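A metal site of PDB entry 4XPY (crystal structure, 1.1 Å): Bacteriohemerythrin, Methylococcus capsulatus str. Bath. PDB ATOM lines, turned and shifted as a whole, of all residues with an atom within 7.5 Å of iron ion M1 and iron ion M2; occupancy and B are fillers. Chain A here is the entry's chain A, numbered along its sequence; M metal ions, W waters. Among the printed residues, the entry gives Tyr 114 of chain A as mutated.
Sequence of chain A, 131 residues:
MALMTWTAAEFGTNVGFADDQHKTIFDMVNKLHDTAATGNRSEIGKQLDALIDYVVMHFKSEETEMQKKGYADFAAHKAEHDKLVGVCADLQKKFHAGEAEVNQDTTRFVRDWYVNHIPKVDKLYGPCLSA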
ATOM      1  N   THR A  13     -23.515  22.184  -1.364  1.00  0.00           N
ATOM      2  CA  THR A  13     -22.684  21.043  -1.746  1.00  0.00           C
ATOM      3  C   THR A  13     -21.952  21.217  -3.036  1.00  0.00           C
ATOM      4  O   THR A  13     -21.143  20.337  -3.399  1.00  0.00           O
ATOM      5  CB  THR A  13     -23.526  19.778  -1.846  1.00  0.00           C
ATOM      6  OG1 THR A  13     -24.436  19.919  -2.944  1.00  0.00           O
ATOM      7  CG2 THR A  13     -24.268  19.401  -0.576  1.00  0.00           C
ATOM      8  N   ALA A  18     -28.765  18.094  -5.486  1.00  0.00           N
ATOM      9  CA  ALA A  18     -28.742  17.758  -4.093  1.00  0.00           C
ATOM     10  C   ALA A  18     -29.130  19.006  -3.269  1.00  0.00           C
ATOM     11  O   ALA A  18     -29.936  18.902  -2.312  1.00  0.00           O
ATOM     12  CB  ALA A  18     -27.362  17.280  -3.691  1.00  0.00           C
ATOM     13  N   ASP A  19     -28.606  20.150  -3.628  1.00  0.00           N
ATOM     14  CA  ASP A  19     -29.040  21.360  -2.944  1.00  0.00           C
ATOM     15  C   ASP A  19     -30.528  21.579  -3.069  1.00  0.00           C
ATOM     16  O   ASP A  19     -31.191  21.987  -2.079  1.00  0.00           O
ATOM     17  CB  ASP A  19     -28.293  22.582  -3.527  1.00  0.00           C
ATOM     18  CG  ASP A  19     -26.832  22.611  -3.164  1.00  0.00           C
ATOM     19  OD1 ASP A  19     -26.317  21.980  -2.246  1.00  0.00           O
ATOM     20  OD2 ASP A  19     -26.135  23.429  -3.927  1.00  0.00           O
ATOM     21  N   GLN A  21     -32.910  19.283  -3.541  1.00  0.00           N
ATOM     22  CA  GLN A  21     -33.617  18.298  -2.738  1.00  0.00           C
ATOM     23  C   GLN A  21     -33.494  18.639  -1.245  1.00  0.00           C
ATOM     24  O   GLN A  21     -34.463  18.471  -0.492  1.00  0.00           O
ATOM     25  CB  GLN A  21     -33.123  16.880  -3.028  1.00  0.00           C
ATOM     26  CG  GLN A  21     -33.422  16.467  -4.476  1.00  0.00           C
ATOM     27  CD  GLN A  21     -32.974  15.069  -4.768  1.00  0.00           C
ATOM     28  OE1 GLN A  21     -32.007  14.552  -4.258  1.00  0.00           O
ATOM     29  NE2 GLN A  21     -33.683  14.386  -5.627  1.00  0.00           N
ATOM     30  N   HIS A  22     -32.326  19.137  -0.832  1.00  0.00           N
ATOM     31  CA  HIS A  22     -32.200  19.563   0.561  1.00  0.00           C
ATOM     32  C   HIS A  22     -33.135  20.695   0.899  1.00  0.00           C
ATOM     33  O   HIS A  22     -33.757  20.716   1.971  1.00  0.00           O
ATOM     34  CB  HIS A  22     -30.756  19.976   0.852  1.00  0.00           C
ATOM     35  CG  HIS A  22     -29.788  18.816   0.774  1.00  0.00           C
ATOM     36  ND1 HIS A  22     -28.445  18.978   0.513  1.00  0.00           N
ATOM     37  CD2 HIS A  22     -29.965  17.477   0.914  1.00  0.00           C
ATOM     38  CE1 HIS A  22     -27.861  17.785   0.524  1.00  0.00           C
ATOM     39  NE2 HIS A  22     -28.746  16.852   0.752  1.00  0.00           N
ATOM     40  N   ILE A  25     -36.511  19.203   1.456  1.00  0.00           N
ATOM     41  CA  ILE A  25     -36.566  18.568   2.777  1.00  0.00           C
ATOM     42  C   ILE A  25     -36.747  19.600   3.868  1.00  0.00           C
ATOM     43  O   ILE A  25     -37.611  19.429   4.754  1.00  0.00           O
ATOM     44  CB  ILE A  25     -35.297  17.704   3.007  1.00  0.00           C
ATOM     45  CG1 ILE A  25     -35.315  16.490   2.151  1.00  0.00           C
ATOM     46  CG2 ILE A  25     -35.151  17.339   4.504  1.00  0.00           C
ATOM     47  CD1 ILE A  25     -34.053  15.722   2.061  1.00  0.00           C
ATOM     48  N   HIS A  58     -34.642  11.283  -2.063  1.00  0.00           N
ATOM     49  CA  HIS A  58     -33.407  12.046  -2.029  1.00  0.00           C
ATOM     50  C   HIS A  58     -32.203  11.107  -1.830  1.00  0.00           C
ATOM     51  O   HIS A  58     -31.182  11.248  -2.521  1.00  0.00           O
ATOM     52  CB  HIS A  58     -33.484  13.104  -0.925  1.00  0.00           C
ATOM     53  CG  HIS A  58     -32.136  13.744  -0.637  1.00  0.00           C
ATOM     54  ND1 HIS A  58     -31.397  14.352  -1.638  1.00  0.00           N
ATOM     55  CD2 HIS A  58     -31.391  13.769   0.485  1.00  0.00           C
ATOM     56  CE1 HIS A  58     -30.253  14.753  -1.086  1.00  0.00           C
ATOM     57  NE2 HIS A  58     -30.212  14.406   0.207  1.00  0.00           N
ATOM     58  N   PHE A  59     -32.308  10.231  -0.880  1.00  0.00           N
ATOM     59  CA  PHE A  59     -31.172   9.338  -0.613  1.00  0.00           C
ATOM     60  C   PHE A  59     -30.929   8.472  -1.824  1.00  0.00           C
ATOM     61  O   PHE A  59     -29.719   8.239  -2.177  1.00  0.00           O
ATOM     62  CB  PHE A  59     -31.457   8.463   0.622  1.00  0.00           C
ATOM     63  CG  PHE A  59     -31.461   9.219   1.920  1.00  0.00           C
ATOM     64  CD1 PHE A  59     -31.999   8.587   3.057  1.00  0.00           C
ATOM     65  CD2 PHE A  59     -30.934  10.511   2.081  1.00  0.00           C
ATOM     66  CE1 PHE A  59     -31.956   9.200   4.276  1.00  0.00           C
ATOM     67  CE2 PHE A  59     -30.925  11.110   3.319  1.00  0.00           C
ATOM     68  CZ  PHE A  59     -31.432  10.470   4.427  1.00  0.00           C
ATOM     69  N   GLU A  62     -28.967  10.630  -4.405  1.00  0.00           N
ATOM     70  CA  GLU A  62     -27.549  10.753  -4.053  1.00  0.00           C
ATOM     71  C   GLU A  62     -26.825   9.437  -4.248  1.00  0.00           C
ATOM     72  O   GLU A  62     -25.687   9.420  -4.794  1.00  0.00           O
ATOM     73  CB  GLU A  62     -27.353  11.127  -2.568  1.00  0.00           C
ATOM     74  CG  GLU A  62     -27.702  12.577  -2.244  1.00  0.00           C
ATOM     75  CD  GLU A  62     -27.266  12.941  -0.821  1.00  0.00           C
ATOM     76  OE1 GLU A  62     -26.809  12.012  -0.124  1.00  0.00           O
ATOM     77  OE2 GLU A  62     -27.418  14.151  -0.470  1.00  0.00           O
ATOM     78  N   GLU A  63     -27.409   8.348  -3.841  1.00  0.00           N
ATOM     79  CA  GLU A  63     -26.724   7.034  -3.916  1.00  0.00           C
ATOM     80  C   GLU A  63     -26.485   6.617  -5.338  1.00  0.00           C
ATOM     81  O   GLU A  63     -25.398   6.091  -5.684  1.00  0.00           O
ATOM     82  CB  GLU A  63     -27.553   5.979  -3.186  1.00  0.00           C
ATOM     83  CG  GLU A  63     -27.565   6.183  -1.697  1.00  0.00           C
ATOM     84  CD  GLU A  63     -28.564   5.459  -0.913  1.00  0.00           C
ATOM     85  OE1 GLU A  63     -29.084   4.401  -1.455  1.00  0.00           O
ATOM     86  OE2 GLU A  63     -28.882   5.789   0.247  1.00  0.00           O
ATOM     87  N   MET A  66     -23.514   8.767  -6.569  1.00  0.00           N
ATOM     88  CA  MET A  66     -22.300   8.378  -5.892  1.00  0.00           C
ATOM     89  C   MET A  66     -21.795   7.067  -6.452  1.00  0.00           C
ATOM     90  O   MET A  66     -20.589   6.897  -6.776  1.00  0.00           O
ATOM     91  CB  MET A  66     -22.472   8.241  -4.376  1.00  0.00           C
ATOM     92  CG  MET A  66     -22.502   9.554  -3.651  1.00  0.00           C
ATOM     93  SD  MET A  66     -22.541   9.390  -1.841  1.00  0.00           S
ATOM     94  CE  MET A  66     -24.221   8.829  -1.528  1.00  0.00           C
ATOM     95  N   HIS A  77     -21.447   6.289   3.375  1.00  0.00           N
ATOM     96  CA  HIS A  77     -22.484   7.329   3.271  1.00  0.00           C
ATOM     97  C   HIS A  77     -23.845   6.681   3.203  1.00  0.00           C
ATOM     98  O   HIS A  77     -24.797   7.067   3.944  1.00  0.00           O
ATOM     99  CB  HIS A  77     -22.131   8.179   2.078  1.00  0.00           C
ATOM    100  CG  HIS A  77     -22.990   9.413   1.928  1.00  0.00           C
ATOM    101  ND1 HIS A  77     -22.456  10.564   1.419  1.00  0.00           N
ATOM    102  CD2 HIS A  77     -24.318   9.683   2.158  1.00  0.00           C
ATOM    103  CE1 HIS A  77     -23.451  11.475   1.357  1.00  0.00           C
ATOM    104  NE2 HIS A  77     -24.585  10.976   1.785  1.00  0.00           N
ATOM    105  N   LYS A  78     -24.001   5.688   2.372  1.00  0.00           N
ATOM    106  CA  LYS A  78     -25.269   4.961   2.277  1.00  0.00           C
ATOM    107  C   LYS A  78     -25.614   4.349   3.600  1.00  0.00           C
ATOM    108  O   LYS A  78     -26.831   4.316   3.964  1.00  0.00           O
ATOM    109  CB  LYS A  78     -25.220   3.900   1.202  1.00  0.00           C
ATOM    110  CG  LYS A  78     -26.526   3.103   1.076  1.00  0.00           C
ATOM    111  CD  LYS A  78     -26.558   2.249  -0.142  1.00  0.00           C
ATOM    112  CE  LYS A  78     -27.749   1.370  -0.274  1.00  0.00           C
ATOM    113  NZ  LYS A  78     -28.070   0.510   0.850  1.00  0.00           N
ATOM    114  N   GLU A  80     -25.167   5.602   6.530  1.00  0.00           N
ATOM    115  CA  GLU A  80     -25.833   6.681   7.286  1.00  0.00           C
ATOM    116  C   GLU A  80     -27.271   6.870   6.833  1.00  0.00           C
ATOM    117  O   GLU A  80     -28.193   6.961   7.686  1.00  0.00           O
ATOM    118  CB  GLU A  80     -25.062   8.025   7.154  1.00  0.00           C
ATOM    119  CG  GLU A  80     -23.585   7.957   7.528  1.00  0.00           C
ATOM    120  CD  GLU A  80     -23.268   7.447   8.910  1.00  0.00           C
ATOM    121  OE1 GLU A  80     -24.097   7.447   9.806  1.00  0.00           O
ATOM    122  OE2 GLU A  80     -22.036   7.029   9.107  1.00  0.00           O
ATOM    123  N   HIS A  81     -27.478   6.918   5.537  1.00  0.00           N
ATOM    124  CA  HIS A  81     -28.846   7.046   4.986  1.00  0.00           C
ATOM    125  C   HIS A  81     -29.724   5.894   5.484  1.00  0.00           C
ATOM    126  O   HIS A  81     -30.850   6.114   5.981  1.00  0.00           O
ATOM    127  CB  HIS A  81     -28.853   6.953   3.505  1.00  0.00           C
ATOM    128  CG  HIS A  81     -28.218   8.134   2.819  1.00  0.00           C
ATOM    129  ND1 HIS A  81     -28.058   8.142   1.443  1.00  0.00           N
ATOM    130  CD2 HIS A  81     -27.801   9.354   3.247  1.00  0.00           C
ATOM    131  CE1 HIS A  81     -27.543   9.342   1.094  1.00  0.00           C
ATOM    132  NE2 HIS A  81     -27.367  10.083   2.177  1.00  0.00           N
ATOM    133  N   TRP A 113     -30.297  15.728  12.505  1.00  0.00           N
ATOM    134  CA  TRP A 113     -29.712  14.784  11.576  1.00  0.00           C
ATOM    135  C   TRP A 113     -29.251  15.509  10.316  1.00  0.00           C
ATOM    136  O   TRP A 113     -28.100  15.308   9.850  1.00  0.00           O
ATOM    137  CB  TRP A 113     -30.702  13.665  11.270  1.00  0.00           C
ATOM    138  CG  TRP A 113     -30.068  12.510  10.583  1.00  0.00           C
ATOM    139  CD1 TRP A 113     -29.619  11.342  11.170  1.00  0.00           C
ATOM    140  CD2 TRP A 113     -29.743  12.387   9.202  1.00  0.00           C
ATOM    141  NE1 TRP A 113     -29.087  10.497  10.229  1.00  0.00           N
ATOM    142  CE2 TRP A 113     -29.141  11.123   9.004  1.00  0.00           C
ATOM    143  CE3 TRP A 113     -29.999  13.181   8.071  1.00  0.00           C
ATOM    144  CZ2 TRP A 113     -28.716  10.681   7.738  1.00  0.00           C
ATOM    145  CZ3 TRP A 113     -29.586  12.723   6.815  1.00  0.00           C
ATOM    146  CH2 TRP A 113     -28.958  11.463   6.667  1.00  0.00           C
ATOM    147  N   TYR A 114     -30.122  16.328   9.717  1.00  0.00           N
ATOM    148  CA  TYR A 114     -29.751  16.995   8.455  1.00  0.00           C
ATOM    149  C   TYR A 114     -28.686  18.025   8.623  1.00  0.00           C
ATOM    150  O   TYR A 114     -27.802  18.171   7.728  1.00  0.00           O
ATOM    151  CB  TYR A 114     -30.986  17.645   7.776  1.00  0.00           C
ATOM    152  CG  TYR A 114     -31.938  16.675   7.302  1.00  0.00           C
ATOM    153  CD1 TYR A 114     -31.655  15.824   6.333  1.00  0.00           C
ATOM    154  CD2 TYR A 114     -33.231  16.753   7.934  1.00  0.00           C
ATOM    155  CE1 TYR A 114     -32.714  14.730   6.085  1.00  0.00           C
ATOM    156  CE2 TYR A 114     -34.222  15.856   7.668  1.00  0.00           C
ATOM    157  CZ  TYR A 114     -33.865  14.827   6.881  1.00  0.00           C
ATOM    158  OH  TYR A 114     -34.877  13.933   6.575  1.00  0.00           O
ATOM    159  N   HIS A 117     -25.577  15.967   8.842  1.00  0.00           N
ATOM    160  CA  HIS A 117     -25.265  15.149   7.673  1.00  0.00           C
ATOM    161  C   HIS A 117     -24.844  15.975   6.482  1.00  0.00           C
ATOM    162  O   HIS A 117     -23.899  15.630   5.771  1.00  0.00           O
ATOM    163  CB  HIS A 117     -26.495  14.326   7.300  1.00  0.00           C
ATOM    164  CG  HIS A 117     -26.265  13.394   6.159  1.00  0.00           C
ATOM    165  ND1 HIS A 117     -25.730  12.122   6.330  1.00  0.00           N
ATOM    166  CD2 HIS A 117     -26.519  13.513   4.841  1.00  0.00           C
ATOM    167  CE1 HIS A 117     -25.698  11.530   5.142  1.00  0.00           C
ATOM    168  NE2 HIS A 117     -26.174  12.318   4.195  1.00  0.00           N
ATOM    169  N   ILE A 118     -25.551  17.089   6.207  1.00  0.00           N
ATOM    170  CA  ILE A 118     -25.280  17.790   4.982  1.00  0.00           C
ATOM    171  C   ILE A 118     -23.839  18.357   4.972  1.00  0.00           C
ATOM    172  O   ILE A 118     -23.097  18.149   4.035  1.00  0.00           O
ATOM    173  CB  ILE A 118     -26.374  18.825   4.646  1.00  0.00           C
ATOM    174  CG1 ILE A 118     -27.670  18.085   4.371  1.00  0.00           C
ATOM    175  CG2 ILE A 118     -25.912  19.672   3.436  1.00  0.00           C
ATOM    176  CD1 ILE A 118     -28.901  18.993   4.321  1.00  0.00           C
ATOM    177  N   VAL A 121     -21.133  15.090   5.684  1.00  0.00           N
ATOM    178  CA  VAL A 121     -21.230  13.906   4.885  1.00  0.00           C
ATOM    179  C   VAL A 121     -21.498  14.308   3.425  1.00  0.00           C
ATOM    180  O   VAL A 121     -20.725  13.955   2.518  1.00  0.00           O
ATOM    181  CB  VAL A 121     -22.280  12.877   5.428  1.00  0.00           C
ATOM    182  CG1 VAL A 121     -22.125  11.586   4.727  1.00  0.00           C
ATOM    183  CG2 VAL A 121     -22.072  12.702   6.935  1.00  0.00           C
ATOM    184  N   ASP A 122     -22.606  15.069   3.180  1.00  0.00           N
ATOM    185  CA  ASP A 122     -22.900  15.403   1.769  1.00  0.00           C
ATOM    186  C   ASP A 122     -21.885  16.311   1.135  1.00  0.00           C
ATOM    187  O   ASP A 122     -21.531  16.152  -0.014  1.00  0.00           O
ATOM    188  CB  ASP A 122     -24.317  16.014   1.635  1.00  0.00           C
ATOM    189  CG  ASP A 122     -25.417  15.039   1.867  1.00  0.00           C
ATOM    190  OD1 ASP A 122     -25.174  13.796   1.808  1.00  0.00           O
ATOM    191  OD2 ASP A 122     -26.573  15.545   2.031  1.00  0.00           O
ATOM    192  N   LYS A 123     -21.404  17.307   1.886  1.00  0.00           N
ATOM    193  CA  LYS A 123     -20.449  18.247   1.181  1.00  0.00           C
ATOM    194  C   LYS A 123     -19.260  17.478   0.648  1.00  0.00           C
ATOM    195  O   LYS A 123     -18.633  17.932  -0.336  1.00  0.00           O
ATOM    196  CB  LYS A 123     -19.974  19.329   2.121  1.00  0.00           C
ATOM    197  CG  LYS A 123     -20.960  20.437   2.368  1.00  0.00           C
ATOM    198  CD  LYS A 123     -20.376  21.579   3.162  1.00  0.00           C
ATOM    199  CE  LYS A 123     -21.345  22.662   3.460  1.00  0.00           C
ATOM    200  NZ  LYS A 123     -20.652  23.828   4.066  1.00  0.00           N
ATOM    201  N   TYR A 125     -19.057  14.866  -1.137  1.00  0.00           N
ATOM    202  CA  TYR A 125     -19.194  14.360  -2.440  1.00  0.00           C
ATOM    203  C   TYR A 125     -19.150  15.454  -3.523  1.00  0.00           C
ATOM    204  O   TYR A 125     -19.206  15.170  -4.664  1.00  0.00           O
ATOM    205  CB  TYR A 125     -20.461  13.475  -2.654  1.00  0.00           C
ATOM    206  CG  TYR A 125     -21.819  14.099  -2.406  1.00  0.00           C
ATOM    207  CD1 TYR A 125     -22.172  15.333  -2.941  1.00  0.00           C
ATOM    208  CD2 TYR A 125     -22.726  13.382  -1.660  1.00  0.00           C
ATOM    209  CE1 TYR A 125     -23.439  15.879  -2.680  1.00  0.00           C
ATOM    210  CE2 TYR A 125     -23.977  13.880  -1.398  1.00  0.00           C
ATOM    211  CZ  TYR A 125     -24.301  15.142  -1.853  1.00  0.00           C
ATOM    212  OH  TYR A 125     -25.551  15.762  -1.592  1.00  0.00           O
HETATM  213 FE    FE M   1     -26.474  12.078   2.036  1.00  0.00          FE
HETATM  214 FE    FE M   2     -28.444  14.779   1.408  1.00  0.00          FE
HETATM  215  O   HOH W   1     -28.227  13.000   2.091  1.00  0.00           O
HETATM  216  O   HOH W   2     -29.722  15.216   3.440  1.00  0.00           O
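Iron ion M1 is bound by water W1 (2.0 Å), the side-chain carboxylate of Asp 122 (2.2 Å), the side-chain carboxylate of Glu 62 (2.2 Å), a ring nitrogen (NE2) of His 81 (2.2 Å), a ring nitrogen (NE2) of His 117 (2.2 Å) and a ring nitrogen (NE2) of His 77 (2.2 Å).
Along chain A the residues within 4 Å of iron ion M1 span positions 62 to 122.
Water W1 is bound to iron ion M2 (1.9 Å). Iron ion M2 is bound by OD2 of Asp 122 (2.1 Å). Iron ion M2 is bound by NE2 of His 58 (2.2 Å). A ring nitrogen (NE2) of His 22 is bound to iron ion M2 (2.2 Å). Iron ion M2 is bound by OE2 of Glu 62. Water W2 is bound to iron ion M2 (2.4 Å). Iron ion M2 has six donor atoms within binding distance.
The side-chain carboxylate of Glu 62 lies close to the side-chain hydroxyl of Tyr 125. A ring nitrogen (ND1) of His 77 is in hydrogen-bond range of the side-chain sulfur (SD) of Met 66 (3.5 Å). OE1 of Gln 21 is in hydrogen-bond range of ND1 of His 58 (2.7 Å). ND1 of His 22 sits close to O of Ala 18 (3.2 Å). ND1 of His 81 sits at hydrogen-bond distance from OE2 of Glu 63 (2.8 Å).
The nearest printed residue that does not touch iron ion M2 is His 117 (4.1 Å).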
